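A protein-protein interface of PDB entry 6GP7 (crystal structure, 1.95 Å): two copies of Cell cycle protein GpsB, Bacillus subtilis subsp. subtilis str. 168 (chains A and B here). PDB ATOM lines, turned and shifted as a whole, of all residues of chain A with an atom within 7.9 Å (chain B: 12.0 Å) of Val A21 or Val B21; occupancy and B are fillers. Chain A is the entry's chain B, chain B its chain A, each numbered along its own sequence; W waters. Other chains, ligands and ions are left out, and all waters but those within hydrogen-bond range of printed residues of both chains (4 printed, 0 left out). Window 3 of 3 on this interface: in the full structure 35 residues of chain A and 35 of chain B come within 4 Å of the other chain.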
ATOM      1  N   THR A  19      17.455 -23.549 -15.675  1.00  0.00           N
ATOM      2  CA  THR A  19      18.067 -22.925 -14.518  1.00  0.00           C
ATOM      3  C   THR A  19      17.037 -22.741 -13.411  1.00  0.00           C
ATOM      4  O   THR A  19      15.829 -22.865 -13.614  1.00  0.00           O
ATOM      5  CB  THR A  19      18.687 -21.580 -14.903  1.00  0.00           C
ATOM      6  OG1 THR A  19      17.739 -20.816 -15.657  1.00  0.00           O
ATOM      7  CG2 THR A  19      19.946 -21.806 -15.756  1.00  0.00           C
ATOM      8  N   GLY A  20      17.544 -22.468 -12.222  1.00  0.00           N
ATOM      9  CA  GLY A  20      16.682 -22.181 -11.092  1.00  0.00           C
ATOM     10  C   GLY A  20      17.504 -21.578  -9.982  1.00  0.00           C
ATOM     11  O   GLY A  20      18.735 -21.545 -10.038  1.00  0.00           O
ATOM     12  N   VAL A  21      16.791 -21.114  -8.956  1.00  0.00           N
ATOM     13  CA  VAL A  21      17.443 -20.560  -7.780  1.00  0.00           C
ATOM     14  C   VAL A  21      18.263 -21.645  -7.093  1.00  0.00           C
ATOM     15  O   VAL A  21      17.846 -22.810  -7.000  1.00  0.00           O
ATOM     16  CB  VAL A  21      16.380 -19.956  -6.847  1.00  0.00           C
ATOM     17  CG1 VAL A  21      15.452 -21.054  -6.265  1.00  0.00           C
ATOM     18  CG2 VAL A  21      17.053 -19.137  -5.720  1.00  0.00           C
ATOM     19  N   ARG A  22      19.463 -21.276  -6.631  1.00  0.00           N
ATOM     20  CA  ARG A  22      20.364 -22.214  -5.948  1.00  0.00           C
ATOM     21  C   ARG A  22      20.657 -23.444  -6.802  1.00  0.00           C
ATOM     22  O   ARG A  22      20.938 -24.527  -6.279  1.00  0.00           O
ATOM     23  CB  ARG A  22      19.825 -22.655  -4.590  1.00  0.00           C
ATOM     24  CG  ARG A  22      19.433 -21.529  -3.692  1.00  0.00           C
ATOM     25  CD  ARG A  22      20.608 -20.692  -3.273  1.00  0.00           C
ATOM     26  NE  ARG A  22      20.215 -19.887  -2.122  1.00  0.00           N
ATOM     27  CZ  ARG A  22      20.999 -19.011  -1.511  1.00  0.00           C
ATOM     28  NH1 ARG A  22      22.232 -18.800  -1.954  1.00  0.00           N
ATOM     29  NH2 ARG A  22      20.538 -18.325  -0.473  1.00  0.00           N
ATOM     30  N   GLY A  23      20.621 -23.286  -8.109  1.00  0.00           N
ATOM     31  CA  GLY A  23      21.064 -24.348  -8.979  1.00  0.00           C
ATOM     32  C   GLY A  23      22.565 -24.525  -8.886  1.00  0.00           C
ATOM     33  O   GLY A  23      23.286 -23.699  -8.330  1.00  0.00           O
ATOM     34  N   TYR A  24      23.043 -25.632  -9.451  1.00  0.00           N
ATOM     35  CA  TYR A  24      24.476 -25.888  -9.459  1.00  0.00           C
ATOM     36  C   TYR A  24      25.189 -24.856 -10.322  1.00  0.00           C
ATOM     37  O   TYR A  24      24.729 -24.523 -11.416  1.00  0.00           O
ATOM     38  CB  TYR A  24      24.766 -27.273 -10.016  1.00  0.00           C
ATOM     39  CG  TYR A  24      24.303 -28.469  -9.213  1.00  0.00           C
ATOM     40  CD1 TYR A  24      24.491 -28.551  -7.838  1.00  0.00           C
ATOM     41  CD2 TYR A  24      23.715 -29.545  -9.861  1.00  0.00           C
ATOM     42  CE1 TYR A  24      24.087 -29.686  -7.123  1.00  0.00           C
ATOM     43  CE2 TYR A  24      23.322 -30.677  -9.164  1.00  0.00           C
ATOM     44  CZ  TYR A  24      23.507 -30.745  -7.809  1.00  0.00           C
ATOM     45  OH  TYR A  24      23.094 -31.880  -7.143  1.00  0.00           O
ATOM     46  N   LYS A  25      26.343 -24.380  -9.850  1.00  0.00           N
ATOM     47  CA  LYS A  25      27.128 -23.421 -10.625  1.00  0.00           C
ATOM     48  C   LYS A  25      27.466 -23.994 -12.004  1.00  0.00           C
ATOM     49  O   LYS A  25      28.015 -25.091 -12.111  1.00  0.00           O
ATOM     50  CB  LYS A  25      28.412 -23.064  -9.868  1.00  0.00           C
ATOM     51  N   GLN A  26      27.145 -23.238 -13.060  1.00  0.00           N
ATOM     52  CA  GLN A  26      27.262 -23.759 -14.423  1.00  0.00           C
ATOM     53  C   GLN A  26      28.685 -24.167 -14.750  1.00  0.00           C
ATOM     54  O   GLN A  26      28.903 -25.173 -15.434  1.00  0.00           O
ATOM     55  CB  GLN A  26      26.789 -22.722 -15.445  1.00  0.00           C
ATOM     56  CG  GLN A  26      25.299 -22.436 -15.407  1.00  0.00           C
ATOM     57  CD  GLN A  26      24.955 -21.274 -14.497  1.00  0.00           C
ATOM     58  OE1 GLN A  26      25.494 -21.142 -13.393  1.00  0.00           O
ATOM     59  NE2 GLN A  26      24.057 -20.413 -14.963  1.00  0.00           N
ATOM     60  N   PHE B  17      28.954 -29.985  -6.306  1.00  0.00           N
ATOM     61  CA  PHE B  17      28.947 -28.779  -7.125  1.00  0.00           C
ATOM     62  C   PHE B  17      28.630 -27.578  -6.256  1.00  0.00           C
ATOM     63  O   PHE B  17      27.722 -27.629  -5.424  1.00  0.00           O
ATOM     64  CB  PHE B  17      27.918 -28.864  -8.253  1.00  0.00           C
ATOM     65  CG  PHE B  17      28.100 -30.047  -9.157  1.00  0.00           C
ATOM     66  CD1 PHE B  17      29.072 -30.032 -10.152  1.00  0.00           C
ATOM     67  CD2 PHE B  17      27.288 -31.170  -9.021  1.00  0.00           C
ATOM     68  CE1 PHE B  17      29.242 -31.133 -11.006  1.00  0.00           C
ATOM     69  CE2 PHE B  17      27.447 -32.266  -9.870  1.00  0.00           C
ATOM     70  CZ  PHE B  17      28.432 -32.249 -10.855  1.00  0.00           C
ATOM     71  N   LYS B  18      29.361 -26.494  -6.457  1.00  0.00           N
ATOM     72  CA  LYS B  18      28.962 -25.250  -5.818  1.00  0.00           C
ATOM     73  C   LYS B  18      27.611 -24.815  -6.368  1.00  0.00           C
ATOM     74  O   LYS B  18      27.217 -25.182  -7.473  1.00  0.00           O
ATOM     75  CB  LYS B  18      30.001 -24.158  -6.065  1.00  0.00           C
ATOM     76  CG  LYS B  18      31.331 -24.386  -5.366  1.00  0.00           C
ATOM     77  N   THR B  19      26.880 -24.041  -5.580  1.00  0.00           N
ATOM     78  CA  THR B  19      25.647 -23.459  -6.081  1.00  0.00           C
ATOM     79  C   THR B  19      25.835 -21.959  -6.269  1.00  0.00           C
ATOM     80  O   THR B  19      26.757 -21.352  -5.723  1.00  0.00           O
ATOM     81  CB  THR B  19      24.474 -23.739  -5.138  1.00  0.00           C
ATOM     82  OG1 THR B  19      24.694 -23.058  -3.902  1.00  0.00           O
ATOM     83  CG2 THR B  19      24.331 -25.242  -4.889  1.00  0.00           C
ATOM     84  N   GLY B  20      24.968 -21.362  -7.082  1.00  0.00           N
ATOM     85  CA  GLY B  20      24.934 -19.926  -7.239  1.00  0.00           C
ATOM     86  C   GLY B  20      23.572 -19.400  -6.833  1.00  0.00           C
ATOM     87  O   GLY B  20      22.660 -20.166  -6.522  1.00  0.00           O
ATOM     88  N   VAL B  21      23.450 -18.067  -6.840  1.00  0.00           N
ATOM     89  CA  VAL B  21      22.119 -17.476  -6.747  1.00  0.00           C
ATOM     90  C   VAL B  21      21.201 -18.140  -7.760  1.00  0.00           C
ATOM     91  O   VAL B  21      20.068 -18.522  -7.451  1.00  0.00           O
ATOM     92  CB  VAL B  21      22.184 -15.951  -6.942  1.00  0.00           C
ATOM     93  CG1 VAL B  21      20.780 -15.362  -7.009  1.00  0.00           C
ATOM     94  CG2 VAL B  21      22.974 -15.308  -5.790  1.00  0.00           C
ATOM     95  N   ARG B  22      21.691 -18.312  -8.987  1.00  0.00           N
ATOM     96  CA  ARG B  22      21.037 -19.148  -9.973  1.00  0.00           C
ATOM     97  C   ARG B  22      22.069 -20.127 -10.514  1.00  0.00           C
ATOM     98  O   ARG B  22      23.270 -19.864 -10.481  1.00  0.00           O
ATOM     99  CB  ARG B  22      20.443 -18.316 -11.134  1.00  0.00           C
ATOM    100  CG  ARG B  22      19.424 -17.275 -10.670  1.00  0.00           C
ATOM    101  CD  ARG B  22      19.008 -16.359 -11.822  1.00  0.00           C
ATOM    102  NE  ARG B  22      18.176 -17.037 -12.824  1.00  0.00           N
ATOM    103  CZ  ARG B  22      18.183 -16.719 -14.115  1.00  0.00           C
ATOM    104  NH1 ARG B  22      18.995 -15.777 -14.543  1.00  0.00           N
ATOM    105  NH2 ARG B  22      17.405 -17.358 -14.985  1.00  0.00           N
ATOM    106  N   GLY B  23      21.588 -21.257 -11.008  1.00  0.00           N
ATOM    107  CA  GLY B  23      22.458 -22.220 -11.655  1.00  0.00           C
ATOM    108  C   GLY B  23      21.603 -23.225 -12.384  1.00  0.00           C
ATOM    109  O   GLY B  23      20.387 -23.064 -12.482  1.00  0.00           O
ATOM    110  N   TYR B  24      22.243 -24.280 -12.882  1.00  0.00           N
ATOM    111  CA  TYR B  24      21.485 -25.379 -13.473  1.00  0.00           C
ATOM    112  C   TYR B  24      20.598 -26.056 -12.425  1.00  0.00           C
ATOM    113  O   TYR B  24      21.056 -26.399 -11.330  1.00  0.00           O
ATOM    114  CB  TYR B  24      22.430 -26.409 -14.083  1.00  0.00           C
ATOM    115  CG  TYR B  24      23.242 -25.959 -15.274  1.00  0.00           C
ATOM    116  CD1 TYR B  24      22.686 -25.188 -16.282  1.00  0.00           C
ATOM    117  CD2 TYR B  24      24.570 -26.365 -15.412  1.00  0.00           C
ATOM    118  CE1 TYR B  24      23.431 -24.815 -17.389  1.00  0.00           C
ATOM    119  CE2 TYR B  24      25.316 -26.010 -16.510  1.00  0.00           C
ATOM    120  CZ  TYR B  24      24.749 -25.229 -17.490  1.00  0.00           C
ATOM    121  OH  TYR B  24      25.496 -24.869 -18.578  1.00  0.00           O
ATOM    122  N   LYS B  25      19.329 -26.281 -12.771  1.00  0.00           N
ATOM    123  CA  LYS B  25      18.387 -26.921 -11.856  1.00  0.00           C
ATOM    124  C   LYS B  25      18.957 -28.233 -11.330  1.00  0.00           C
ATOM    125  O   LYS B  25      19.346 -29.112 -12.102  1.00  0.00           O
ATOM    126  CB  LYS B  25      17.054 -27.181 -12.549  1.00  0.00           C
ATOM    127  CG  LYS B  25      15.863 -27.301 -11.587  1.00  0.00           C
ATOM    128  CD  LYS B  25      15.376 -25.895 -11.210  1.00  0.00           C
ATOM    129  CE  LYS B  25      14.127 -25.931 -10.341  1.00  0.00           C
ATOM    130  NZ  LYS B  25      13.725 -24.548  -9.948  1.00  0.00           N
ATOM    131  N   GLN B  26      19.016 -28.358 -10.008  1.00  0.00           N
ATOM    132  CA  GLN B  26      19.737 -29.493  -9.423  1.00  0.00           C
ATOM    133  C   GLN B  26      19.064 -30.811  -9.764  1.00  0.00           C
ATOM    134  O   GLN B  26      19.742 -31.813 -10.030  1.00  0.00           O
ATOM    135  CB  GLN B  26      19.841 -29.329  -7.909  1.00  0.00           C
ATOM    136  CG  GLN B  26      20.770 -28.214  -7.478  1.00  0.00           C
ATOM    137  CD  GLN B  26      21.055 -28.251  -6.008  1.00  0.00           C
ATOM    138  OE1 GLN B  26      21.002 -29.313  -5.378  1.00  0.00           O
ATOM    139  NE2 GLN B  26      21.372 -27.092  -5.442  1.00  0.00           N
ATOM    140  N   GLU B  27      17.730 -30.825  -9.770  1.00  0.00           N
ATOM    141  CA  GLU B  27      16.999 -32.032 -10.100  1.00  0.00           C
ATOM    142  C   GLU B  27      17.368 -32.536 -11.490  1.00  0.00           C
ATOM    143  O   GLU B  27      17.622 -33.732 -11.674  1.00  0.00           O
ATOM    144  CB  GLU B  27      15.495 -31.776 -10.017  1.00  0.00           C
ATOM    145  CG  GLU B  27      14.667 -32.981 -10.405  1.00  0.00           C
ATOM    146  CD  GLU B  27      13.177 -32.746 -10.238  1.00  0.00           C
ATOM    147  OE1 GLU B  27      12.778 -31.602  -9.926  1.00  0.00           O
ATOM    148  OE2 GLU B  27      12.401 -33.711 -10.421  1.00  0.00           O
ATOM    149  N   ASP B  28      17.415 -31.633 -12.471  1.00  0.00           N
ATOM    150  CA  ASP B  28      17.682 -32.021 -13.850  1.00  0.00           C
ATOM    151  C   ASP B  28      19.116 -32.508 -14.035  1.00  0.00           C
ATOM    152  O   ASP B  28      19.356 -33.452 -14.802  1.00  0.00           O
ATOM    153  CB  ASP B  28      17.409 -30.849 -14.788  1.00  0.00           C
ATOM    154  CG  ASP B  28      15.976 -30.349 -14.692  1.00  0.00           C
ATOM    155  OD1 ASP B  28      15.317 -30.602 -13.660  1.00  0.00           O
ATOM    156  OD2 ASP B  28      15.510 -29.713 -15.654  1.00  0.00           O
ATOM    157  N   VAL B  29      20.083 -31.829 -13.406  1.00  0.00           N
ATOM    158  CA  VAL B  29      21.473 -32.268 -13.489  1.00  0.00           C
ATOM    159  C   VAL B  29      21.623 -33.661 -12.876  1.00  0.00           C
ATOM    160  O   VAL B  29      22.229 -34.555 -13.478  1.00  0.00           O
ATOM    161  CB  VAL B  29      22.411 -31.246 -12.824  1.00  0.00           C
ATOM    162  CG1 VAL B  29      23.850 -31.815 -12.717  1.00  0.00           C
ATOM    163  CG2 VAL B  29      22.440 -29.931 -13.654  1.00  0.00           C
ATOM    164  N   ASP B  30      21.059 -33.868 -11.680  1.00  0.00           N
ATOM    165  CA  ASP B  30      21.215 -35.160 -10.999  1.00  0.00           C
ATOM    166  C   ASP B  30      20.590 -36.287 -11.805  1.00  0.00           C
ATOM    167  O   ASP B  30      21.133 -37.396 -11.861  1.00  0.00           O
ATOM    168  CB  ASP B  30      20.553 -35.159  -9.622  1.00  0.00           C
ATOM    169  CG  ASP B  30      21.262 -34.306  -8.599  1.00  0.00           C
ATOM    170  OD1 ASP B  30      22.399 -33.858  -8.844  1.00  0.00           O
ATOM    171  OD2 ASP B  30      20.649 -34.088  -7.525  1.00  0.00           O
HETATM  172  O   HOH W   1      24.003 -19.539  -3.506  1.00  0.00           O
HETATM  173  O   HOH W   2      13.889 -21.432  -9.339  1.00  0.00           O
HETATM  174  O   HOH W   3      16.070 -24.160  -8.201  1.00  0.00           O
HETATM  175  O   HOH W   4      20.436 -32.253  -5.676  1.00  0.00           O
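N of Gly A20 lies within hydrogen-bond range of O of Gly B23, 2.9 Å away.
O of Gly B20 sits close to N of Arg A22 (3.4 Å).
The backbone NH (N) of Arg A22 sits at hydrogen-bond distance from the backbone carbonyl oxygen (O) of Val B21 (2.9 Å).
The backbone carbonyl oxygen of Arg A22 lies within hydrogen-bond range of the side-chain amide nitrogen of Gln B26.
The backbone carbonyl oxygen of Gly A23 is in hydrogen-bond range of the backbone NH of Gly B20 (3.1 Å).
The backbone carbonyl oxygen (O) of Tyr B24 sits at hydrogen-bond distance from the backbone NH (N) of Tyr A24 (2.8 Å).
The side-chain hydroxyl (OH) of Tyr A24 is in hydrogen-bond range of the side-chain carboxylate (OD1) of Asp B30, 2.7 Å away.
The backbone NH (N) of Lys A25 sits at hydrogen-bond distance from the backbone carbonyl oxygen (O) of Lys B18 (2.7 Å).
O of Gly B23 touches CA of Thr A19, at 3.1 Å.
Gly A20 touches Lys B25 (CA to CD, 3.9 Å).
Gly A23 touches Thr B19.
CA of Gly B23 touches C of Gly A23 (3.6 Å).
O of Tyr B24 touches CA of Gly A23 (3.1 Å).
CE1 of Tyr A24 touches CD of Gln B26, 3.5 Å away.
Tyr A24 touches Val B29 (CD2 to CG1, 3.7 Å).
CA of Thr B19 touches N of Lys A25 (3.9 Å).
CA of Gly B23 touches OE1 of Gln A26, 3.7 Å away.
Gln A26 touches Tyr B24.
Of chain B, only Arg B22 (3.5 Å), Gly B23 (3.1 Å) and Lys B25 (3.9 Å) come within 4 Å of Thr A19.
Of the printed residues of chain B, Val A21 touches Val B21 (3.3 Å).
Of the printed residues of chain B, Tyr A24 touches Phe B17, Lys B18, Gly B23, Tyr B24, Gln B26, Val B29 and Asp B30.
Printed residues of chain B within 4 Å of Lys A25: Lys B18 and Thr B19.
Gly B20 touches just these residues of chain A: Arg A22 (3.1 Å) and Gly A23 (3.1 Å).
Val B21 touches two residues of chain A.
Glu B27 touches none of the printed residues of chain A.
The nearest residue of chain B that does not touch Val A21 is Arg B22 (4.4 Å).
Printed residues of chain A that touch a printed residue of chain B: Thr A19, Gly A20, Val A21, Arg A22, Gly A23, Tyr A24, Lys A25 and Gln A26.
Hydrophobic or aromatic side chains of chain A within 4 Å of the printed part of chain B: Val A21 and Tyr A24.
Among the printed residues, 27 pairs touch across the chains.
Thr A19 touches Lys B25, and with the chains exchanged Lys A25 touches Thr B19.
Gly A20 touches Gly B23, and with the chains exchanged Gly A23 touches Gly B20.
Val A21 touches its own counterpart, Val B21.
Tyr A24 touches Gln B26, and with the chains exchanged Gln A26 touches Tyr B24.
8 positions are printed for both chains.
Water W1 lies within hydrogen-bond range of the guanidinium group (NH1) of Arg A22 (2.5 Å) and the backbone carbonyl oxygen (O) of Gly B20 (3.4 Å).
Water W3 lies within hydrogen-bond range of O of Val A21 and NZ of Lys B25.
Water W4 lies within hydrogen-bond range of the side-chain carboxylate of Asp B30 (2.6 Å), the side-chain amide oxygen of Gln B26 (3.0 Å) and the side-chain hydroxyl of Tyr A24 (3.1 Å).
Water W2 bridges the backbone NH of Val A21 (2.9 Å) and the side-chain amino group of Lys B25 (3.2 Å).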
